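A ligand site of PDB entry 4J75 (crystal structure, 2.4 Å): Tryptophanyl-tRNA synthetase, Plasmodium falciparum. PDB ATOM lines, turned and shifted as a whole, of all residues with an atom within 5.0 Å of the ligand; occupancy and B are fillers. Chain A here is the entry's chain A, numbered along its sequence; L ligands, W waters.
The side-chain amide nitrogen (NE2) of Gln 233 is in hydrogen-bond range of the side-chain carboxylate (OD2) of Asp 232 (3.1 Å). The side-chain amide nitrogen (NE2) of Gln 206 lies within hydrogen-bond range of the side-chain amide oxygen (OE1) of Gln 233. OE1 of Gln 206 is in hydrogen-bond range of OH of Tyr 202 (2.7 Å). The side-chain amide oxygen of Gln 118 is in hydrogen-bond range of the side-chain hydroxyl of Tyr 202, 3.5 Å away. The backbone NH (N) of Ser 120 lies within hydrogen-bond range of the backbone carbonyl oxygen (O) of Arg 86, 3.0 Å away. The guanidinium group (NH1) of Arg 86 lies within hydrogen-bond range of a ring nitrogen (NE2) of His 97. The side-chain sulfur (SD) of Met 270 sits at hydrogen-bond distance from the backbone NH (N) of Gly 96, at 3.7 Å. The backbone carbonyl oxygen (O) of Pro 228 lies within hydrogen-bond range of the side-chain hydroxyl (OG1) of Thr 84, at 2.8 Å.
An oxygen (O5) of the ligand sits at hydrogen-bond distance from the side-chain carboxylate (OD1) of Asp 232 (2.6 Å). An oxygen (O1) of the ligand sits at hydrogen-bond distance from the backbone NH of Gly 87. OE1 of Gln 206 lies within hydrogen-bond range of N6 of the ligand (2.8 Å). N of Met 260 is in hydrogen-bond range of N3 of the ligand (2.8 Å). The backbone carbonyl oxygen (O) of Met 260 sits at hydrogen-bond distance from a nitrogen (N4) of the ligand (3.0 Å). OE1 of Glu 123 lies within salt-bridge range of N6 of the ligand. N7 of the ligand sits at hydrogen-bond distance from OE1 of Gln 118 (2.9 Å). The backbone NH (N) of Gly 230 sits at hydrogen-bond distance from an oxygen (O5) of the ligand (2.9 Å). An oxygen (O1) of the ligand lies within salt-bridge range of the guanidinium group (NH1) of Arg 86, at 3.0 Å. The side-chain hydroxyl (OH) of Tyr 83 is in hydrogen-bond range of a nitrogen (N7) of the ligand, at 3.1 Å. N6 of the ligand sits close to OE1 of Gln 233. A nitrogen (N4) of the ligand lies within hydrogen-bond range of the backbone carbonyl oxygen (O) of Met 270 (3.4 Å). An oxygen (O7) of the ligand sits close to the side-chain amino group (NZ) of Lys 124, at 3.4 Å.
The backbone carbonyl oxygen (O) of Gly 96 sits close to a nitrogen (N2) of the ligand (3.2 Å). Merely in contact with the ligand: Lys 269, Gly 85, Phe 259, Pro 100, Phe 237, Ser 120, Val 258, Thr 84, Tyr 202, Gln 229 and His 97. Hydrophobic or aromatic side chains within 4 Å of the ligand: Tyr 83, His 97, Pro 100, Phe 237, Phe 259, Met 260 and Met 270. Of the 32 residues printed, 24 come within 4 Å of the ligand. The nearest printed residue that does not touch the ligand is Ile 99 (4.03 Å).
Water W1 bridges an oxygen (O2) of the ligand (2.7 Å) and the side-chain amino group of Lys 124 (3.0 Å). Water W5 lies within hydrogen-bond range of OG1 of Thr 84 (2.6 Å), O6 of the ligand (2.7 Å) and O of Gly 85 (2.9 Å). Water W2 lies within hydrogen-bond range of O2 of the ligand (2.8 Å), O of Gly 87 (2.8 Å) and NH1 of Arg 86 (3.2 Å). Water W4 lies within hydrogen-bond range of an oxygen (O2) of the ligand (2.9 Å), the side-chain carboxylate of Asp 232 (3.0 Å) and the side-chain amino group of Lys 269 (3.2 Å). Water W6 bridges NE2 of His 97 (3.0 Å) and O2 of the ligand (3.0 Å). Water W3 lies within hydrogen-bond range of OH of Tyr 236 (2.6 Å), OE2 of Glu 123 (2.8 Å) and N6 of the ligand (3.0 Å).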
ATOM      1  N   TYR A  83       9.071 -25.273   2.216  1.00  0.00           N
ATOM      2  CA  TYR A  83      10.248 -24.439   1.984  1.00  0.00           C
ATOM      3  C   TYR A  83      10.927 -24.899   0.715  1.00  0.00           C
ATOM      4  O   TYR A  83      11.202 -26.089   0.544  1.00  0.00           O
ATOM      5  CB  TYR A  83      11.208 -24.514   3.186  1.00  0.00           C
ATOM      6  CG  TYR A  83      12.627 -24.040   2.912  1.00  0.00           C
ATOM      7  CD1 TYR A  83      12.883 -22.880   2.195  1.00  0.00           C
ATOM      8  CD2 TYR A  83      13.723 -24.754   3.414  1.00  0.00           C
ATOM      9  CE1 TYR A  83      14.180 -22.446   1.964  1.00  0.00           C
ATOM     10  CE2 TYR A  83      15.020 -24.321   3.173  1.00  0.00           C
ATOM     11  CZ  TYR A  83      15.241 -23.175   2.449  1.00  0.00           C
ATOM     12  OH  TYR A  83      16.517 -22.746   2.210  1.00  0.00           O
ATOM     13  N   THR A  84      11.175 -23.956  -0.192  1.00  0.00           N
ATOM     14  CA  THR A  84      12.040 -24.226  -1.310  1.00  0.00           C
ATOM     15  C   THR A  84      12.762 -22.941  -1.699  1.00  0.00           C
ATOM     16  O   THR A  84      12.523 -21.896  -1.102  1.00  0.00           O
ATOM     17  CB  THR A  84      11.252 -24.810  -2.499  1.00  0.00           C
ATOM     18  OG1 THR A  84      12.180 -25.461  -3.392  1.00  0.00           O
ATOM     19  CG2 THR A  84      10.468 -23.739  -3.228  1.00  0.00           C
ATOM     20  N   GLY A  85      13.662 -23.005  -2.669  1.00  0.00           N
ATOM     21  CA  GLY A  85      14.460 -21.837  -3.021  1.00  0.00           C
ATOM     22  C   GLY A  85      14.966 -21.747  -4.434  1.00  0.00           C
ATOM     23  O   GLY A  85      14.841 -22.689  -5.238  1.00  0.00           O
ATOM     24  N   ARG A  86      15.518 -20.588  -4.738  1.00  0.00           N
ATOM     25  CA  ARG A  86      16.060 -20.278  -6.054  1.00  0.00           C
ATOM     26  C   ARG A  86      17.331 -19.470  -5.878  1.00  0.00           C
ATOM     27  O   ARG A  86      17.343 -18.470  -5.163  1.00  0.00           O
ATOM     28  CB  ARG A  86      15.018 -19.497  -6.858  1.00  0.00           C
ATOM     29  CG  ARG A  86      15.546 -18.669  -8.014  1.00  0.00           C
ATOM     30  CD  ARG A  86      16.012 -19.531  -9.157  1.00  0.00           C
ATOM     31  NE  ARG A  86      16.628 -18.743 -10.214  1.00  0.00           N
ATOM     32  CZ  ARG A  86      17.513 -19.186 -11.095  1.00  0.00           C
ATOM     33  NH1 ARG A  86      17.952 -20.453 -11.069  1.00  0.00           N
ATOM     34  NH2 ARG A  86      18.000 -18.361 -12.006  1.00  0.00           N
ATOM     35  N   GLY A  87      18.401 -19.910  -6.540  1.00  0.00           N
ATOM     36  CA  GLY A  87      19.638 -19.154  -6.618  1.00  0.00           C
ATOM     37  C   GLY A  87      19.631 -18.306  -7.881  1.00  0.00           C
ATOM     38  O   GLY A  87      19.670 -18.848  -8.997  1.00  0.00           O
ATOM     39  N   HIS A  94      14.423 -21.301 -16.861  1.00  0.00           N
ATOM     40  CA  HIS A  94      13.832 -22.226 -17.827  1.00  0.00           C
ATOM     41  C   HIS A  94      12.794 -23.122 -17.134  1.00  0.00           C
ATOM     42  O   HIS A  94      12.564 -23.011 -15.921  1.00  0.00           O
ATOM     43  CB  HIS A  94      14.920 -23.057 -18.532  1.00  0.00           C
ATOM     44  CG  HIS A  94      15.879 -23.733 -17.612  1.00  0.00           C
ATOM     45  ND1 HIS A  94      15.497 -24.719 -16.722  1.00  0.00           N
ATOM     46  CD2 HIS A  94      17.219 -23.582 -17.445  1.00  0.00           C
ATOM     47  CE1 HIS A  94      16.542 -25.122 -16.037  1.00  0.00           C
ATOM     48  NE2 HIS A  94      17.606 -24.468 -16.455  1.00  0.00           N
ATOM     49  N   GLY A  96      12.636 -26.300 -16.332  1.00  0.00           N
ATOM     50  CA  GLY A  96      13.158 -27.111 -15.238  1.00  0.00           C
ATOM     51  C   GLY A  96      13.167 -26.411 -13.899  1.00  0.00           C
ATOM     52  O   GLY A  96      12.837 -27.031 -12.868  1.00  0.00           O
ATOM     53  N   HIS A  97      13.527 -25.120 -13.891  1.00  0.00           N
ATOM     54  CA  HIS A  97      13.546 -24.318 -12.643  1.00  0.00           C
ATOM     55  C   HIS A  97      12.153 -24.182 -12.049  1.00  0.00           C
ATOM     56  O   HIS A  97      12.011 -23.959 -10.853  1.00  0.00           O
ATOM     57  CB  HIS A  97      14.109 -22.907 -12.882  1.00  0.00           C
ATOM     58  CG  HIS A  97      15.577 -22.869 -13.166  1.00  0.00           C
ATOM     59  ND1 HIS A  97      16.134 -22.082 -14.168  1.00  0.00           N
ATOM     60  CD2 HIS A  97      16.622 -23.511 -12.587  1.00  0.00           C
ATOM     61  CE1 HIS A  97      17.442 -22.245 -14.189  1.00  0.00           C
ATOM     62  NE2 HIS A  97      17.760 -23.109 -13.238  1.00  0.00           N
ATOM     63  N   ILE A  99       9.708 -26.614 -12.105  1.00  0.00           N
ATOM     64  CA  ILE A  99       9.178 -27.889 -11.600  1.00  0.00           C
ATOM     65  C   ILE A  99       8.945 -27.846 -10.088  1.00  0.00           C
ATOM     66  O   ILE A  99       7.841 -28.155  -9.630  1.00  0.00           O
ATOM     67  CB  ILE A  99      10.079 -29.093 -11.963  1.00  0.00           C
ATOM     68  CG1 ILE A  99      10.191 -29.254 -13.485  1.00  0.00           C
ATOM     69  CG2 ILE A  99       9.570 -30.389 -11.336  1.00  0.00           C
ATOM     70  CD1 ILE A  99       8.874 -29.249 -14.233  1.00  0.00           C
ATOM     71  N   PRO A 100       9.952 -27.474  -9.306  1.00  0.00           N
ATOM     72  CA  PRO A 100       9.731 -27.411  -7.867  1.00  0.00           C
ATOM     73  C   PRO A 100       8.648 -26.412  -7.492  1.00  0.00           C
ATOM     74  O   PRO A 100       7.893 -26.643  -6.552  1.00  0.00           O
ATOM     75  CB  PRO A 100      11.090 -26.951  -7.310  1.00  0.00           C
ATOM     76  CG  PRO A 100      12.062 -27.210  -8.386  1.00  0.00           C
ATOM     77  CD  PRO A 100      11.303 -27.014  -9.654  1.00  0.00           C
ATOM     78  N   PHE A 101       8.583 -25.303  -8.223  1.00  0.00           N
ATOM     79  CA  PHE A 101       7.648 -24.232  -7.915  1.00  0.00           C
ATOM     80  C   PHE A 101       6.212 -24.573  -8.308  1.00  0.00           C
ATOM     81  O   PHE A 101       5.294 -24.290  -7.540  1.00  0.00           O
ATOM     82  CB  PHE A 101       8.131 -22.917  -8.522  1.00  0.00           C
ATOM     83  CG  PHE A 101       9.345 -22.355  -7.824  1.00  0.00           C
ATOM     84  CD1 PHE A 101       9.214 -21.747  -6.586  1.00  0.00           C
ATOM     85  CD2 PHE A 101      10.605 -22.495  -8.367  1.00  0.00           C
ATOM     86  CE1 PHE A 101      10.317 -21.257  -5.924  1.00  0.00           C
ATOM     87  CE2 PHE A 101      11.727 -22.009  -7.706  1.00  0.00           C
ATOM     88  CZ  PHE A 101      11.578 -21.388  -6.479  1.00  0.00           C
ATOM     89  N   GLN A 118      13.204 -18.997  -0.391  1.00  0.00           N
ATOM     90  CA  GLN A 118      14.472 -18.325  -0.241  1.00  0.00           C
ATOM     91  C   GLN A 118      15.041 -17.983  -1.582  1.00  0.00           C
ATOM     92  O   GLN A 118      15.139 -18.840  -2.450  1.00  0.00           O
ATOM     93  CB  GLN A 118      15.467 -19.240   0.469  1.00  0.00           C
ATOM     94  CG  GLN A 118      16.869 -18.659   0.639  1.00  0.00           C
ATOM     95  CD  GLN A 118      17.754 -19.579   1.448  1.00  0.00           C
ATOM     96  OE1 GLN A 118      18.183 -20.632   0.980  1.00  0.00           O
ATOM     97  NE2 GLN A 118      18.008 -19.215   2.693  1.00  0.00           N
ATOM     98  N   SER A 120      18.488 -17.126  -2.755  1.00  0.00           N
ATOM     99  CA  SER A 120      19.836 -17.174  -2.236  1.00  0.00           C
ATOM    100  C   SER A 120      20.732 -16.248  -3.054  1.00  0.00           C
ATOM    101  O   SER A 120      21.676 -16.701  -3.716  1.00  0.00           O
ATOM    102  CB  SER A 120      20.338 -18.611  -2.207  1.00  0.00           C
ATOM    103  OG  SER A 120      20.251 -19.223  -3.479  1.00  0.00           O
ATOM    104  N   GLU A 123      24.312 -16.499  -1.919  1.00  0.00           N
ATOM    105  CA  GLU A 123      24.985 -17.618  -2.547  1.00  0.00           C
ATOM    106  C   GLU A 123      25.586 -17.189  -3.879  1.00  0.00           C
ATOM    107  O   GLU A 123      26.760 -17.399  -4.128  1.00  0.00           O
ATOM    108  CB  GLU A 123      24.011 -18.771  -2.779  1.00  0.00           C
ATOM    109  CG  GLU A 123      24.674 -20.039  -3.291  1.00  0.00           C
ATOM    110  CD  GLU A 123      23.700 -21.030  -3.912  1.00  0.00           C
ATOM    111  OE1 GLU A 123      22.445 -20.878  -3.793  1.00  0.00           O
ATOM    112  OE2 GLU A 123      24.210 -21.975  -4.527  1.00  0.00           O
ATOM    113  N   LYS A 124      24.760 -16.611  -4.748  1.00  0.00           N
ATOM    114  CA  LYS A 124      25.174 -16.400  -6.116  1.00  0.00           C
ATOM    115  C   LYS A 124      26.125 -15.234  -6.256  1.00  0.00           C
ATOM    116  O   LYS A 124      26.973 -15.225  -7.150  1.00  0.00           O
ATOM    117  CB  LYS A 124      23.974 -16.258  -7.037  1.00  0.00           C
ATOM    118  CG  LYS A 124      23.099 -17.503  -7.065  1.00  0.00           C
ATOM    119  CD  LYS A 124      23.895 -18.769  -7.375  1.00  0.00           C
ATOM    120  CE  LYS A 124      23.005 -19.992  -7.414  1.00  0.00           C
ATOM    121  NZ  LYS A 124      23.779 -21.220  -7.716  1.00  0.00           N
ATOM    122  N   TYR A 202      27.936 -20.274   3.494  1.00  0.00           N
ATOM    123  CA  TYR A 202      26.576 -20.220   2.915  1.00  0.00           C
ATOM    124  C   TYR A 202      25.630 -21.397   3.247  1.00  0.00           C
ATOM    125  O   TYR A 202      24.452 -21.164   3.504  1.00  0.00           O
ATOM    126  CB  TYR A 202      26.604 -20.041   1.394  1.00  0.00           C
ATOM    127  CG  TYR A 202      25.229 -20.270   0.834  1.00  0.00           C
ATOM    128  CD1 TYR A 202      24.227 -19.330   1.039  1.00  0.00           C
ATOM    129  CD2 TYR A 202      24.898 -21.455   0.200  1.00  0.00           C
ATOM    130  CE1 TYR A 202      22.930 -19.554   0.595  1.00  0.00           C
ATOM    131  CE2 TYR A 202      23.609 -21.690  -0.244  1.00  0.00           C
ATOM    132  CZ  TYR A 202      22.633 -20.726  -0.044  1.00  0.00           C
ATOM    133  OH  TYR A 202      21.341 -20.929  -0.481  1.00  0.00           O
ATOM    134  N   GLN A 206      21.252 -21.806   3.732  1.00  0.00           N
ATOM    135  CA  GLN A 206      20.284 -22.626   2.993  1.00  0.00           C
ATOM    136  C   GLN A 206      19.547 -23.597   3.925  1.00  0.00           C
ATOM    137  O   GLN A 206      18.391 -23.955   3.676  1.00  0.00           O
ATOM    138  CB  GLN A 206      20.961 -23.414   1.838  1.00  0.00           C
ATOM    139  CG  GLN A 206      19.978 -24.239   1.030  1.00  0.00           C
ATOM    140  CD  GLN A 206      20.335 -24.420  -0.437  1.00  0.00           C
ATOM    141  OE1 GLN A 206      20.917 -23.546  -1.087  1.00  0.00           O
ATOM    142  NE2 GLN A 206      19.974 -25.576  -0.972  1.00  0.00           N
ATOM    143  N   VAL A 227      10.401 -29.845   2.283  1.00  0.00           N
ATOM    144  CA  VAL A 227      11.366 -29.179   1.406  1.00  0.00           C
ATOM    145  C   VAL A 227      11.444 -29.853   0.028  1.00  0.00           C
ATOM    146  O   VAL A 227      12.273 -30.742  -0.171  1.00  0.00           O
ATOM    147  CB  VAL A 227      12.780 -29.147   2.043  1.00  0.00           C
ATOM    148  CG1 VAL A 227      13.730 -28.295   1.230  1.00  0.00           C
ATOM    149  CG2 VAL A 227      12.701 -28.613   3.466  1.00  0.00           C
ATOM    150  N   PRO A 228      10.590 -29.423  -0.925  1.00  0.00           N
ATOM    151  CA  PRO A 228      10.685 -29.943  -2.279  1.00  0.00           C
ATOM    152  C   PRO A 228      11.913 -29.371  -2.983  1.00  0.00           C
ATOM    153  O   PRO A 228      12.224 -28.177  -2.841  1.00  0.00           O
ATOM    154  CB  PRO A 228       9.385 -29.449  -2.957  1.00  0.00           C
ATOM    155  CG  PRO A 228       8.509 -29.003  -1.855  1.00  0.00           C
ATOM    156  CD  PRO A 228       9.445 -28.509  -0.789  1.00  0.00           C
ATOM    157  N   GLN A 229      12.576 -30.205  -3.760  1.00  0.00           N
ATOM    158  CA  GLN A 229      13.848 -29.856  -4.343  1.00  0.00           C
ATOM    159  C   GLN A 229      14.194 -30.838  -5.427  1.00  0.00           C
ATOM    160  O   GLN A 229      13.716 -31.977  -5.432  1.00  0.00           O
ATOM    161  CB  GLN A 229      14.938 -29.917  -3.292  1.00  0.00           C
ATOM    162  CG  GLN A 229      15.125 -31.310  -2.712  1.00  0.00           C
ATOM    163  CD  GLN A 229      15.888 -31.326  -1.402  1.00  0.00           C
ATOM    164  OE1 GLN A 229      17.080 -31.641  -1.360  1.00  0.00           O
ATOM    165  NE2 GLN A 229      15.193 -31.028  -0.317  1.00  0.00           N
ATOM    166  N   GLY A 230      15.013 -30.384  -6.373  1.00  0.00           N
ATOM    167  CA  GLY A 230      15.663 -31.291  -7.272  1.00  0.00           C
ATOM    168  C   GLY A 230      16.746 -31.989  -6.469  1.00  0.00           C
ATOM    169  O   GLY A 230      17.219 -31.485  -5.444  1.00  0.00           O
ATOM    170  N   ILE A 231      17.123 -33.166  -6.951  1.00  0.00           N
ATOM    171  CA  ILE A 231      18.002 -34.060  -6.205  1.00  0.00           C
ATOM    172  C   ILE A 231      19.398 -33.435  -5.928  1.00  0.00           C
ATOM    173  O   ILE A 231      20.096 -33.864  -5.016  1.00  0.00           O
ATOM    174  CB  ILE A 231      18.074 -35.433  -6.939  1.00  0.00           C
ATOM    175  CG1 ILE A 231      18.574 -36.527  -6.007  1.00  0.00           C
ATOM    176  CG2 ILE A 231      18.935 -35.354  -8.183  1.00  0.00           C
ATOM    177  CD1 ILE A 231      17.553 -37.020  -5.003  1.00  0.00           C
ATOM    178  N   ASP A 232      19.775 -32.403  -6.701  1.00  0.00           N
ATOM    179  CA  ASP A 232      21.076 -31.732  -6.493  1.00  0.00           C
ATOM    180  C   ASP A 232      21.189 -30.936  -5.190  1.00  0.00           C
ATOM    181  O   ASP A 232      22.293 -30.609  -4.773  1.00  0.00           O
ATOM    182  CB  ASP A 232      21.458 -30.822  -7.678  1.00  0.00           C
ATOM    183  CG  ASP A 232      20.476 -29.678  -7.907  1.00  0.00           C
ATOM    184  OD1 ASP A 232      19.271 -29.862  -7.637  1.00  0.00           O
ATOM    185  OD2 ASP A 232      20.909 -28.603  -8.366  1.00  0.00           O
ATOM    186  N   GLN A 233      20.068 -30.612  -4.564  1.00  0.00           N
ATOM    187  CA  GLN A 233      20.074 -29.868  -3.299  1.00  0.00           C
ATOM    188  C   GLN A 233      20.232 -30.765  -2.071  1.00  0.00           C
ATOM    189  O   GLN A 233      20.415 -30.287  -0.963  1.00  0.00           O
ATOM    190  CB  GLN A 233      18.792 -29.063  -3.132  1.00  0.00           C
ATOM    191  CG  GLN A 233      18.503 -28.126  -4.284  1.00  0.00           C
ATOM    192  CD  GLN A 233      19.656 -27.173  -4.527  1.00  0.00           C
ATOM    193  OE1 GLN A 233      20.132 -26.508  -3.619  1.00  0.00           O
ATOM    194  NE2 GLN A 233      20.128 -27.128  -5.772  1.00  0.00           N
ATOM    195  N   TYR A 236      22.741 -30.409   1.160  1.00  0.00           N
ATOM    196  CA  TYR A 236      22.364 -29.457   2.197  1.00  0.00           C
ATOM    197  C   TYR A 236      21.428 -30.071   3.218  1.00  0.00           C
ATOM    198  O   TYR A 236      21.566 -29.840   4.415  1.00  0.00           O
ATOM    199  CB  TYR A 236      21.637 -28.260   1.603  1.00  0.00           C
ATOM    200  CG  TYR A 236      22.472 -27.402   0.705  1.00  0.00           C
ATOM    201  CD1 TYR A 236      23.329 -26.446   1.227  1.00  0.00           C
ATOM    202  CD2 TYR A 236      22.374 -27.518  -0.676  1.00  0.00           C
ATOM    203  CE1 TYR A 236      24.084 -25.633   0.400  1.00  0.00           C
ATOM    204  CE2 TYR A 236      23.118 -26.705  -1.523  1.00  0.00           C
ATOM    205  CZ  TYR A 236      23.963 -25.763  -0.969  1.00  0.00           C
ATOM    206  OH  TYR A 236      24.697 -24.955  -1.794  1.00  0.00           O
ATOM    207  N   PHE A 237      20.435 -30.825   2.735  1.00  0.00           N
ATOM    208  CA  PHE A 237      19.342 -31.212   3.613  1.00  0.00           C
ATOM    209  C   PHE A 237      19.578 -32.542   4.294  1.00  0.00           C
ATOM    210  O   PHE A 237      19.029 -32.796   5.364  1.00  0.00           O
ATOM    211  CB  PHE A 237      18.012 -31.124   2.847  1.00  0.00           C
ATOM    212  CG  PHE A 237      17.738 -29.730   2.374  1.00  0.00           C
ATOM    213  CD1 PHE A 237      17.516 -28.714   3.294  1.00  0.00           C
ATOM    214  CD2 PHE A 237      17.809 -29.406   1.027  1.00  0.00           C
ATOM    215  CE1 PHE A 237      17.305 -27.411   2.876  1.00  0.00           C
ATOM    216  CE2 PHE A 237      17.597 -28.104   0.599  1.00  0.00           C
ATOM    217  CZ  PHE A 237      17.349 -27.112   1.523  1.00  0.00           C
ATOM    218  N   SER A 257      12.836 -34.364  -6.675  1.00  0.00           N
ATOM    219  CA  SER A 257      12.436 -34.494  -8.065  1.00  0.00           C
ATOM    220  C   SER A 257      13.590 -35.026  -8.905  1.00  0.00           C
ATOM    221  O   SER A 257      14.762 -34.739  -8.610  1.00  0.00           O
ATOM    222  CB  SER A 257      12.041 -33.120  -8.599  1.00  0.00           C
ATOM    223  OG  SER A 257      11.675 -33.203  -9.966  1.00  0.00           O
ATOM    224  N   VAL A 258      13.273 -35.777  -9.957  1.00  0.00           N
ATOM    225  CA  VAL A 258      14.223 -35.993 -11.067  1.00  0.00           C
ATOM    226  C   VAL A 258      14.490 -34.660 -11.782  1.00  0.00           C
ATOM    227  O   VAL A 258      13.778 -33.672 -11.561  1.00  0.00           O
ATOM    228  CB  VAL A 258      13.704 -36.985 -12.121  1.00  0.00           C
ATOM    229  CG1 VAL A 258      13.465 -38.357 -11.505  1.00  0.00           C
ATOM    230  CG2 VAL A 258      12.440 -36.469 -12.803  1.00  0.00           C
ATOM    231  N   PHE A 259      15.514 -34.614 -12.621  1.00  0.00           N
ATOM    232  CA  PHE A 259      15.717 -33.437 -13.467  1.00  0.00           C
ATOM    233  C   PHE A 259      14.912 -33.562 -14.751  1.00  0.00           C
ATOM    234  O   PHE A 259      14.877 -34.629 -15.377  1.00  0.00           O
ATOM    235  CB  PHE A 259      17.204 -33.267 -13.826  1.00  0.00           C
ATOM    236  CG  PHE A 259      18.078 -33.012 -12.621  1.00  0.00           C
ATOM    237  CD1 PHE A 259      17.794 -31.987 -11.747  1.00  0.00           C
ATOM    238  CD2 PHE A 259      19.181 -33.827 -12.351  1.00  0.00           C
ATOM    239  CE1 PHE A 259      18.586 -31.763 -10.624  1.00  0.00           C
ATOM    240  CE2 PHE A 259      19.970 -33.614 -11.237  1.00  0.00           C
ATOM    241  CZ  PHE A 259      19.680 -32.568 -10.375  1.00  0.00           C
ATOM    242  N   MET A 260      14.225 -32.494 -15.124  1.00  0.00           N
ATOM    243  CA  MET A 260      13.658 -32.383 -16.467  1.00  0.00           C
ATOM    244  C   MET A 260      14.826 -32.314 -17.448  1.00  0.00           C
ATOM    245  O   MET A 260      15.679 -31.435 -17.321  1.00  0.00           O
ATOM    246  CB  MET A 260      12.788 -31.132 -16.614  1.00  0.00           C
ATOM    247  CG  MET A 260      11.918 -31.144 -17.854  1.00  0.00           C
ATOM    248  SD  MET A 260      10.822 -29.731 -17.942  1.00  0.00           S
ATOM    249  CE  MET A 260       9.823 -30.209 -19.358  1.00  0.00           C
ATOM    250  N   LYS A 269      20.277 -32.827 -18.014  1.00  0.00           N
ATOM    251  CA  LYS A 269      19.538 -31.840 -17.227  1.00  0.00           C
ATOM    252  C   LYS A 269      19.395 -30.561 -18.071  1.00  0.00           C
ATOM    253  O   LYS A 269      20.343 -30.135 -18.731  1.00  0.00           O
ATOM    254  CB  LYS A 269      20.291 -31.546 -15.937  1.00  0.00           C
ATOM    255  CG  LYS A 269      19.675 -30.501 -15.023  1.00  0.00           C
ATOM    256  CD  LYS A 269      20.744 -29.988 -14.059  1.00  0.00           C
ATOM    257  CE  LYS A 269      20.138 -29.150 -12.954  1.00  0.00           C
ATOM    258  NZ  LYS A 269      21.195 -28.487 -12.144  1.00  0.00           N
ATOM    259  N   MET A 270      18.212 -29.960 -18.041  1.00  0.00           N
ATOM    260  CA  MET A 270      18.017 -28.642 -18.654  1.00  0.00           C
ATOM    261  C   MET A 270      18.774 -27.605 -17.811  1.00  0.00           C
ATOM    262  O   MET A 270      18.525 -27.489 -16.597  1.00  0.00           O
ATOM    263  CB  MET A 270      16.529 -28.312 -18.718  1.00  0.00           C
ATOM    264  CG  MET A 270      16.227 -27.027 -19.471  1.00  0.00           C
ATOM    265  SD  MET A 270      14.472 -26.653 -19.522  1.00  0.00           S
ATOM    266  CE  MET A 270      13.916 -27.758 -20.814  1.00  0.00           C
HETATM  267  P1  LIG L   1      18.688 -23.283  -8.407  1.00  0.00           P
HETATM  268  O1  LIG L   1      18.220 -21.841  -8.409  1.00  0.00           O
HETATM  269  O2  LIG L   1      19.927 -23.685  -9.196  1.00  0.00           O
HETATM  270  O3  LIG L   1      17.483 -24.296  -8.789  1.00  0.00           O
HETATM  271  C1  LIG L   1      16.186 -24.054  -8.243  1.00  0.00           C
HETATM  272  C2  LIG L   1      15.426 -25.369  -8.101  1.00  0.00           C
HETATM  273  O4  LIG L   1      15.160 -25.991  -9.371  1.00  0.00           O
HETATM  274  C3  LIG L   1      15.660 -27.348  -9.369  1.00  0.00           C
HETATM  275  N1  LIG L   1      16.090 -27.669 -10.745  1.00  0.00           N
HETATM  276  C4  LIG L   1      15.459 -28.533 -11.533  1.00  0.00           C
HETATM  277  N2  LIG L   1      14.385 -29.350 -11.390  1.00  0.00           N
HETATM  278  C5  LIG L   1      13.966 -30.145 -12.400  1.00  0.00           C
HETATM  279  N3  LIG L   1      14.585 -30.181 -13.606  1.00  0.00           N
HETATM  280  C6  LIG L   1      15.670 -29.423 -13.886  1.00  0.00           C
HETATM  281  N4  LIG L   1      16.274 -29.476 -15.089  1.00  0.00           N
HETATM  282  C7  LIG L   1      16.178 -28.519 -12.822  1.00  0.00           C
HETATM  283  N5  LIG L   1      17.188 -27.634 -12.686  1.00  0.00           N
HETATM  284  C8  LIG L   1      17.117 -27.121 -11.433  1.00  0.00           C
HETATM  285  C9  LIG L   1      16.740 -27.372  -8.291  1.00  0.00           C
HETATM  286  O5  LIG L   1      16.915 -28.674  -7.759  1.00  0.00           O
HETATM  287  C10 LIG L   1      16.198 -26.381  -7.256  1.00  0.00           C
HETATM  288  O6  LIG L   1      15.299 -26.994  -6.328  1.00  0.00           O
HETATM  289  N6  LIG L   1      20.928 -23.258  -3.846  1.00  0.00           N
HETATM  290  C11 LIG L   1      19.693 -23.386  -4.587  1.00  0.00           C
HETATM  291  C12 LIG L   1      18.630 -22.396  -4.161  1.00  0.00           C
HETATM  292  C13 LIG L   1      17.968 -22.817  -2.886  1.00  0.00           C
HETATM  293  C14 LIG L   1      17.086 -23.968  -2.641  1.00  0.00           C
HETATM  294  C15 LIG L   1      16.715 -23.882  -1.225  1.00  0.00           C
HETATM  295  C16 LIG L   1      16.596 -24.970  -3.455  1.00  0.00           C
HETATM  296  C17 LIG L   1      18.065 -22.152  -1.680  1.00  0.00           C
HETATM  297  N7  LIG L   1      17.328 -22.780  -0.732  1.00  0.00           N
HETATM  298  C18 LIG L   1      15.868 -24.853  -0.698  1.00  0.00           C
HETATM  299  C19 LIG L   1      15.755 -25.925  -2.870  1.00  0.00           C
HETATM  300  C20 LIG L   1      15.407 -25.863  -1.513  1.00  0.00           C
HETATM  301  C21 LIG L   1      19.891 -23.113  -6.027  1.00  0.00           C
HETATM  302  O7  LIG L   1      20.802 -22.406  -6.471  1.00  0.00           O
HETATM  303  O8  LIG L   1      18.896 -23.723  -6.876  1.00  0.00           O
HETATM  304  O   HOH W   1      22.478 -23.787  -8.409  1.00  0.00           O
HETATM  305  O   HOH W   2      20.883 -21.189  -9.902  1.00  0.00           O
HETATM  306  O   HOH W   3      23.552 -24.671  -4.152  1.00  0.00           O
HETATM  307  O   HOH W   4      19.855 -26.402 -10.138  1.00  0.00           O
HETATM  308  O   HOH W   5      13.445 -25.146  -5.623  1.00  0.00           O
HETATM  309  O   HOH W   6      20.464 -23.579 -12.113  1.00  0.00           O
